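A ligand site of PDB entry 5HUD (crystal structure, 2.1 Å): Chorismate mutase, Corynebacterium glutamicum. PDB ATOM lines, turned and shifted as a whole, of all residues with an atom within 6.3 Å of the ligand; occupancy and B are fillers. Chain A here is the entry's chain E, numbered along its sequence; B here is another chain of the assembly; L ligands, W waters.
An oxygen (O3) of the ligand is in hydrogen-bond range of the side-chain hydroxyl of Ser 39 (2.5 Å). The guanidinium group of Arg 18 of chain B is in salt-bridge range of an oxygen (O6) of the ligand (2.6 Å). An oxygen (O4) of the ligand lies within salt-bridge range of the guanidinium group of Arg 35 (2.7 Å). NH2 of Arg 46 lies within salt-bridge range of O5 of the ligand (2.8 Å). The side-chain carboxylate (OE2) of Glu 59 lies within hydrogen-bond range of an oxygen (O1) of the ligand (2.9 Å). N of Val 55 lies within hydrogen-bond range of O1 of the ligand. The backbone carbonyl oxygen (O) of Val 55 lies within hydrogen-bond range of an oxygen (O1) of the ligand (3.4 Å).
The guanidinium group (NE) of Arg 35 lies within salt-bridge range of the side-chain carboxylate (OD1) of Asp 25 of chain B. O of Arg 53 lies within hydrogen-bond range of NH1 of Arg 46 (2.9 Å). The guanidinium group (NH2) of Arg 86 is in salt-bridge range of the side-chain carboxylate (OE1) of Glu 59 (2.7 Å).
CG2 of Ile 42 touches C7 of the ligand (3.5 Å). CA of Leu 54 touches O1 of the ligand (3.4 Å). CG of Arg 58 touches C3 of the ligand, 3.6 Å away. Ile 62 touches the ligand (CD1 to O4, 3.5 Å). Leu 82 touches the ligand (CD2 to O4, 3.4 Å). CG of Arg 86 touches C6 of the ligand, 3.5 Å away.
Water W1 bridges NH1 of Arg 58 (2.7 Å) and O6 of the ligand (2.9 Å). Water W2 lies within hydrogen-bond range of the backbone carbonyl oxygen (O) of Ser 39 (2.8 Å), an oxygen (O2) of the ligand (3.4 Å) and the backbone NH (N) of Gly 43 (3.4 Å).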
ATOM      1  N   ARG A  35     -16.649  35.893   4.670  1.00  0.00           N
ATOM      2  CA  ARG A  35     -16.572  34.625   5.422  1.00  0.00           C
ATOM      3  C   ARG A  35     -15.392  34.588   6.419  1.00  0.00           C
ATOM      4  O   ARG A  35     -15.560  34.284   7.586  1.00  0.00           O
ATOM      5  CB  ARG A  35     -16.487  33.434   4.467  1.00  0.00           C
ATOM      6  CG  ARG A  35     -16.867  32.120   5.133  1.00  0.00           C
ATOM      7  CD  ARG A  35     -16.221  30.925   4.448  1.00  0.00           C
ATOM      8  NE  ARG A  35     -16.557  29.685   5.157  1.00  0.00           N
ATOM      9  CZ  ARG A  35     -15.937  29.236   6.258  1.00  0.00           C
ATOM     10  NH1 ARG A  35     -16.376  28.110   6.817  1.00  0.00           N
ATOM     11  NH2 ARG A  35     -14.916  29.902   6.819  1.00  0.00           N
ATOM     12  N   ILE A  38     -15.643  36.806   9.391  1.00  0.00           N
ATOM     13  CA  ILE A  38     -16.619  36.300  10.350  1.00  0.00           C
ATOM     14  C   ILE A  38     -16.010  35.138  11.128  1.00  0.00           C
ATOM     15  O   ILE A  38     -16.215  35.046  12.351  1.00  0.00           O
ATOM     16  CB  ILE A  38     -17.953  35.892   9.695  1.00  0.00           C
ATOM     17  CG1 ILE A  38     -18.656  37.130   9.169  1.00  0.00           C
ATOM     18  CG2 ILE A  38     -18.871  35.194  10.690  1.00  0.00           C
ATOM     19  CD1 ILE A  38     -19.832  36.815   8.274  1.00  0.00           C
ATOM     20  N   SER A  39     -15.277  34.274  10.436  1.00  0.00           N
ATOM     21  CA  SER A  39     -14.660  33.136  11.072  1.00  0.00           C
ATOM     22  C   SER A  39     -13.700  33.623  12.126  1.00  0.00           C
ATOM     23  O   SER A  39     -13.791  33.203  13.275  1.00  0.00           O
ATOM     24  CB  SER A  39     -13.928  32.245  10.071  1.00  0.00           C
ATOM     25  OG  SER A  39     -13.320  31.144  10.733  1.00  0.00           O
ATOM     26  N   GLN A  40     -12.798  34.512  11.753  1.00  0.00           N
ATOM     27  CA  GLN A  40     -11.820  35.069  12.696  1.00  0.00           C
ATOM     28  C   GLN A  40     -12.564  35.638  13.924  1.00  0.00           C
ATOM     29  O   GLN A  40     -12.239  35.267  15.065  1.00  0.00           O
ATOM     30  CB  GLN A  40     -10.958  36.145  12.043  1.00  0.00           C
ATOM     31  CG  GLN A  40      -9.924  35.594  11.061  1.00  0.00           C
ATOM     32  CD  GLN A  40      -9.493  36.572   9.965  1.00  0.00           C
ATOM     33  OE1 GLN A  40     -10.266  37.449   9.563  1.00  0.00           O
ATOM     34  NE2 GLN A  40      -8.286  36.410   9.457  1.00  0.00           N
ATOM     35  N   ILE A  42     -15.487  34.960  15.137  1.00  0.00           N
ATOM     36  CA  ILE A  42     -15.954  33.850  15.978  1.00  0.00           C
ATOM     37  C   ILE A  42     -14.798  33.296  16.824  1.00  0.00           C
ATOM     38  O   ILE A  42     -14.994  32.955  17.992  1.00  0.00           O
ATOM     39  CB  ILE A  42     -16.547  32.682  15.159  1.00  0.00           C
ATOM     40  CG1 ILE A  42     -17.843  33.116  14.484  1.00  0.00           C
ATOM     41  CG2 ILE A  42     -16.855  31.476  16.053  1.00  0.00           C
ATOM     42  CD1 ILE A  42     -18.341  32.143  13.433  1.00  0.00           C
ATOM     43  N   GLY A  43     -13.627  33.187  16.210  1.00  0.00           N
ATOM     44  CA  GLY A  43     -12.433  32.669  16.862  1.00  0.00           C
ATOM     45  C   GLY A  43     -11.986  33.484  18.035  1.00  0.00           C
ATOM     46  O   GLY A  43     -11.686  32.939  19.109  1.00  0.00           O
ATOM     47  N   ARG A  46     -14.659  33.240  20.965  1.00  0.00           N
ATOM     48  CA  ARG A  46     -14.545  31.992  21.715  1.00  0.00           C
ATOM     49  C   ARG A  46     -13.267  31.914  22.547  1.00  0.00           C
ATOM     50  O   ARG A  46     -13.300  31.413  23.683  1.00  0.00           O
ATOM     51  CB  ARG A  46     -14.631  30.763  20.790  1.00  0.00           C
ATOM     52  CG  ARG A  46     -14.528  29.430  21.542  1.00  0.00           C
ATOM     53  CD  ARG A  46     -14.719  28.196  20.672  1.00  0.00           C
ATOM     54  NE  ARG A  46     -13.972  28.292  19.415  1.00  0.00           N
ATOM     55  CZ  ARG A  46     -14.497  28.442  18.202  1.00  0.00           C
ATOM     56  NH1 ARG A  46     -13.684  28.534  17.152  1.00  0.00           N
ATOM     57  NH2 ARG A  46     -15.809  28.507  18.008  1.00  0.00           N
ATOM     58  N   ARG A  53      -9.425  27.295  20.067  1.00  0.00           N
ATOM     59  CA  ARG A  53      -9.272  27.887  18.730  1.00  0.00           C
ATOM     60  C   ARG A  53     -10.173  27.163  17.716  1.00  0.00           C
ATOM     61  O   ARG A  53     -10.896  27.820  16.956  1.00  0.00           O
ATOM     62  CB  ARG A  53      -7.798  27.854  18.308  1.00  0.00           C
ATOM     63  CG  ARG A  53      -7.506  28.570  17.015  1.00  0.00           C
ATOM     64  CD  ARG A  53      -6.037  28.557  16.681  1.00  0.00           C
ATOM     65  NE  ARG A  53      -5.284  29.344  17.660  1.00  0.00           N
ATOM     66  CZ  ARG A  53      -5.160  30.672  17.660  1.00  0.00           C
ATOM     67  NH1 ARG A  53      -5.736  31.439  16.741  1.00  0.00           N
ATOM     68  NH2 ARG A  53      -4.430  31.257  18.612  1.00  0.00           N
ATOM     69  N   LEU A  54     -10.162  25.837  17.722  1.00  0.00           N
ATOM     70  CA  LEU A  54     -10.861  25.024  16.728  1.00  0.00           C
ATOM     71  C   LEU A  54     -11.988  24.198  17.359  1.00  0.00           C
ATOM     72  O   LEU A  54     -11.914  23.804  18.535  1.00  0.00           O
ATOM     73  CB  LEU A  54      -9.894  24.041  16.065  1.00  0.00           C
ATOM     74  CG  LEU A  54      -8.512  24.553  15.630  1.00  0.00           C
ATOM     75  CD1 LEU A  54      -7.558  23.394  15.455  1.00  0.00           C
ATOM     76  CD2 LEU A  54      -8.598  25.362  14.366  1.00  0.00           C
ATOM     77  N   VAL A  55     -13.032  23.937  16.575  1.00  0.00           N
ATOM     78  CA  VAL A  55     -14.110  23.046  16.953  1.00  0.00           C
ATOM     79  C   VAL A  55     -14.190  22.018  15.829  1.00  0.00           C
ATOM     80  O   VAL A  55     -14.508  22.379  14.701  1.00  0.00           O
ATOM     81  CB  VAL A  55     -15.442  23.801  17.127  1.00  0.00           C
ATOM     82  CG1 VAL A  55     -16.567  22.874  17.587  1.00  0.00           C
ATOM     83  CG2 VAL A  55     -15.247  24.940  18.126  1.00  0.00           C
ATOM     84  N   HIS A  56     -13.907  20.757  16.159  1.00  0.00           N
ATOM     85  CA  HIS A  56     -13.643  19.708  15.179  1.00  0.00           C
ATOM     86  C   HIS A  56     -14.917  19.271  14.472  1.00  0.00           C
ATOM     87  O   HIS A  56     -15.005  19.323  13.244  1.00  0.00           O
ATOM     88  CB  HIS A  56     -12.963  18.505  15.867  1.00  0.00           C
ATOM     89  CG  HIS A  56     -12.536  17.412  14.929  1.00  0.00           C
ATOM     90  ND1 HIS A  56     -11.628  17.617  13.912  1.00  0.00           N
ATOM     91  CD2 HIS A  56     -12.863  16.096  14.882  1.00  0.00           C
ATOM     92  CE1 HIS A  56     -11.435  16.475  13.262  1.00  0.00           C
ATOM     93  NE2 HIS A  56     -12.159  15.538  13.845  1.00  0.00           N
ATOM     94  N   ARG A  58     -17.597  20.776  14.043  1.00  0.00           N
ATOM     95  CA  ARG A  58     -18.072  21.845  13.208  1.00  0.00           C
ATOM     96  C   ARG A  58     -17.301  21.859  11.900  1.00  0.00           C
ATOM     97  O   ARG A  58     -17.916  21.975  10.844  1.00  0.00           O
ATOM     98  CB  ARG A  58     -17.972  23.186  13.946  1.00  0.00           C
ATOM     99  CG  ARG A  58     -18.362  24.433  13.143  1.00  0.00           C
ATOM    100  CD  ARG A  58     -19.778  24.401  12.582  1.00  0.00           C
ATOM    101  NE  ARG A  58     -19.996  25.574  11.732  1.00  0.00           N
ATOM    102  CZ  ARG A  58     -21.061  25.802  10.958  1.00  0.00           C
ATOM    103  NH1 ARG A  58     -21.108  26.912  10.226  1.00  0.00           N
ATOM    104  NH2 ARG A  58     -22.068  24.941  10.881  1.00  0.00           N
ATOM    105  N   GLU A  59     -15.979  21.727  11.959  1.00  0.00           N
ATOM    106  CA  GLU A  59     -15.142  21.674  10.731  1.00  0.00           C
ATOM    107  C   GLU A  59     -15.466  20.461   9.856  1.00  0.00           C
ATOM    108  O   GLU A  59     -15.664  20.601   8.648  1.00  0.00           O
ATOM    109  CB  GLU A  59     -13.659  21.669  11.067  1.00  0.00           C
ATOM    110  CG  GLU A  59     -13.210  22.950  11.746  1.00  0.00           C
ATOM    111  CD  GLU A  59     -11.744  23.254  11.586  1.00  0.00           C
ATOM    112  OE1 GLU A  59     -11.015  22.442  10.999  1.00  0.00           O
ATOM    113  OE2 GLU A  59     -11.309  24.333  12.031  1.00  0.00           O
ATOM    114  N   ILE A  62     -18.947  20.967   7.903  1.00  0.00           N
ATOM    115  CA  ILE A  62     -18.763  21.826   6.726  1.00  0.00           C
ATOM    116  C   ILE A  62     -18.080  21.066   5.584  1.00  0.00           C
ATOM    117  O   ILE A  62     -18.617  21.013   4.472  1.00  0.00           O
ATOM    118  CB  ILE A  62     -17.935  23.084   7.040  1.00  0.00           C
ATOM    119  CG1 ILE A  62     -18.722  24.023   7.971  1.00  0.00           C
ATOM    120  CG2 ILE A  62     -17.551  23.823   5.759  1.00  0.00           C
ATOM    121  CD1 ILE A  62     -17.843  24.982   8.756  1.00  0.00           C
ATOM    122  N   LEU A  81     -10.992  27.475   3.095  1.00  0.00           N
ATOM    123  CA  LEU A  81     -11.780  28.423   3.870  1.00  0.00           C
ATOM    124  C   LEU A  81     -11.460  28.275   5.364  1.00  0.00           C
ATOM    125  O   LEU A  81     -11.325  29.288   6.053  1.00  0.00           O
ATOM    126  CB  LEU A  81     -13.283  28.295   3.598  1.00  0.00           C
ATOM    127  CG  LEU A  81     -13.738  28.569   2.165  1.00  0.00           C
ATOM    128  CD1 LEU A  81     -15.236  28.409   2.068  1.00  0.00           C
ATOM    129  CD2 LEU A  81     -13.322  29.927   1.655  1.00  0.00           C
ATOM    130  N   LEU A  82     -11.296  27.045   5.838  1.00  0.00           N
ATOM    131  CA  LEU A  82     -10.972  26.819   7.254  1.00  0.00           C
ATOM    132  C   LEU A  82      -9.597  27.379   7.616  1.00  0.00           C
ATOM    133  O   LEU A  82      -9.450  28.097   8.603  1.00  0.00           O
ATOM    134  CB  LEU A  82     -11.077  25.352   7.599  1.00  0.00           C
ATOM    135  CG  LEU A  82     -12.495  24.816   7.472  1.00  0.00           C
ATOM    136  CD1 LEU A  82     -12.554  23.302   7.665  1.00  0.00           C
ATOM    137  CD2 LEU A  82     -13.431  25.525   8.432  1.00  0.00           C
ATOM    138  N   MET A  84      -8.117  29.737   6.039  1.00  0.00           N
ATOM    139  CA  MET A  84      -8.321  31.194   6.000  1.00  0.00           C
ATOM    140  C   MET A  84      -8.990  31.704   7.279  1.00  0.00           C
ATOM    141  O   MET A  84      -8.543  32.691   7.858  1.00  0.00           O
ATOM    142  CB  MET A  84      -9.138  31.601   4.776  1.00  0.00           C
ATOM    143  CG  MET A  84      -8.320  31.487   3.503  1.00  0.00           C
ATOM    144  SD  MET A  84      -9.104  32.129   2.021  1.00  0.00           S
ATOM    145  CE  MET A  84      -8.655  33.867   2.107  1.00  0.00           C
ATOM    146  N   GLY A  85     -10.017  30.999   7.737  1.00  0.00           N
ATOM    147  CA  GLY A  85     -10.759  31.406   8.909  1.00  0.00           C
ATOM    148  C   GLY A  85      -9.925  31.364  10.187  1.00  0.00           C
ATOM    149  O   GLY A  85      -9.651  32.393  10.797  1.00  0.00           O
ATOM    150  N   ARG A  86      -9.501  30.160  10.555  1.00  0.00           N
ATOM    151  CA  ARG A  86      -8.898  29.923  11.874  1.00  0.00           C
ATOM    152  C   ARG A  86      -7.388  29.769  11.817  1.00  0.00           C
ATOM    153  O   ARG A  86      -6.758  29.530  12.833  1.00  0.00           O
ATOM    154  CB  ARG A  86      -9.583  28.737  12.599  1.00  0.00           C
ATOM    155  CG  ARG A  86      -9.894  27.478  11.776  1.00  0.00           C
ATOM    156  CD  ARG A  86      -8.646  26.759  11.265  1.00  0.00           C
ATOM    157  NE  ARG A  86      -8.928  25.340  10.984  1.00  0.00           N
ATOM    158  CZ  ARG A  86      -8.180  24.528  10.223  1.00  0.00           C
ATOM    159  NH1 ARG A  86      -7.084  24.962   9.594  1.00  0.00           N
ATOM    160  NH2 ARG A  86      -8.561  23.255  10.078  1.00  0.00           N
ATOM    161  N   ILE B  14     -22.261  33.593  18.504  1.00  0.00           N
ATOM    162  CA  ILE B  14     -21.547  32.638  17.658  1.00  0.00           C
ATOM    163  C   ILE B  14     -22.521  31.884  16.750  1.00  0.00           C
ATOM    164  O   ILE B  14     -22.248  31.734  15.558  1.00  0.00           O
ATOM    165  CB  ILE B  14     -20.637  31.672  18.487  1.00  0.00           C
ATOM    166  CG1 ILE B  14     -19.366  32.420  18.911  1.00  0.00           C
ATOM    167  CG2 ILE B  14     -20.270  30.413  17.701  1.00  0.00           C
ATOM    168  CD1 ILE B  14     -18.422  31.636  19.793  1.00  0.00           C
ATOM    169  N   ARG B  18     -22.262  31.905  12.732  1.00  0.00           N
ATOM    170  CA  ARG B  18     -22.242  30.647  11.936  1.00  0.00           C
ATOM    171  C   ARG B  18     -23.367  30.547  10.908  1.00  0.00           C
ATOM    172  O   ARG B  18     -23.189  30.003   9.819  1.00  0.00           O
ATOM    173  CB  ARG B  18     -22.328  29.420  12.846  1.00  0.00           C
ATOM    174  CG  ARG B  18     -21.050  29.155  13.635  1.00  0.00           C
ATOM    175  CD  ARG B  18     -21.150  27.859  14.406  1.00  0.00           C
ATOM    176  NE  ARG B  18     -19.922  27.556  15.112  1.00  0.00           N
ATOM    177  CZ  ARG B  18     -19.780  26.576  16.008  1.00  0.00           C
ATOM    178  NH1 ARG B  18     -18.602  26.397  16.608  1.00  0.00           N
ATOM    179  NH2 ARG B  18     -20.805  25.789  16.330  1.00  0.00           N
ATOM    180  N   ILE B  21     -22.050  32.447   8.052  1.00  0.00           N
ATOM    181  CA  ILE B  21     -21.061  31.609   7.318  1.00  0.00           C
ATOM    182  C   ILE B  21     -21.783  30.638   6.400  1.00  0.00           C
ATOM    183  O   ILE B  21     -21.446  30.520   5.218  1.00  0.00           O
ATOM    184  CB  ILE B  21     -20.058  30.860   8.260  1.00  0.00           C
ATOM    185  CG1 ILE B  21     -19.005  31.846   8.770  1.00  0.00           C
ATOM    186  CG2 ILE B  21     -19.354  29.688   7.549  1.00  0.00           C
ATOM    187  CD1 ILE B  21     -18.202  31.368   9.948  1.00  0.00           C
ATOM    188  N   ASP B  25     -21.392  30.201   2.576  1.00  0.00           N
ATOM    189  CA  ASP B  25     -20.998  28.918   1.984  1.00  0.00           C
ATOM    190  C   ASP B  25     -21.913  28.501   0.838  1.00  0.00           C
ATOM    191  O   ASP B  25     -21.413  28.110  -0.220  1.00  0.00           O
ATOM    192  CB  ASP B  25     -20.788  27.849   3.043  1.00  0.00           C
ATOM    193  CG  ASP B  25     -19.517  28.117   3.902  1.00  0.00           C
ATOM    194  OD1 ASP B  25     -18.688  29.005   3.502  1.00  0.00           O
ATOM    195  OD2 ASP B  25     -19.342  27.460   4.975  1.00  0.00           O
HETATM  196  C1  LIG L   1     -14.808  27.974  11.551  1.00  0.00           C
HETATM  197  C2  LIG L   1     -15.429  26.627  11.864  1.00  0.00           C
HETATM  198  C3  LIG L   1     -15.057  25.903  12.937  1.00  0.00           C
HETATM  199  C4  LIG L   1     -14.022  26.365  13.966  1.00  0.00           C
HETATM  200  O1  LIG L   1     -12.979  25.382  14.094  1.00  0.00           O
HETATM  201  C5  LIG L   1     -13.469  27.747  13.635  1.00  0.00           C
HETATM  202  C6  LIG L   1     -13.391  27.973  12.109  1.00  0.00           C
HETATM  203  O2  LIG L   1     -14.256  28.768  14.302  1.00  0.00           O
HETATM  204  C7  LIG L   1     -15.528  29.156  13.728  1.00  0.00           C
HETATM  205  C8  LIG L   1     -15.602  29.096  12.197  1.00  0.00           C
HETATM  206  C9  LIG L   1     -14.856  28.263  10.072  1.00  0.00           C
HETATM  207  O3  LIG L   1     -13.999  29.022   9.559  1.00  0.00           O
HETATM  208  O4  LIG L   1     -15.812  27.807   9.398  1.00  0.00           O
HETATM  209  C10 LIG L   1     -16.638  28.361  14.360  1.00  0.00           C
HETATM  210  O5  LIG L   1     -16.380  27.740  15.404  1.00  0.00           O
HETATM  211  O6  LIG L   1     -17.783  28.327  13.861  1.00  0.00           O
HETATM  212  O   HOH W   1     -18.837  28.007  11.125  1.00  0.00           O
HETATM  213  O   HOH W   2     -11.945  31.222  13.978  1.00  0.00           O
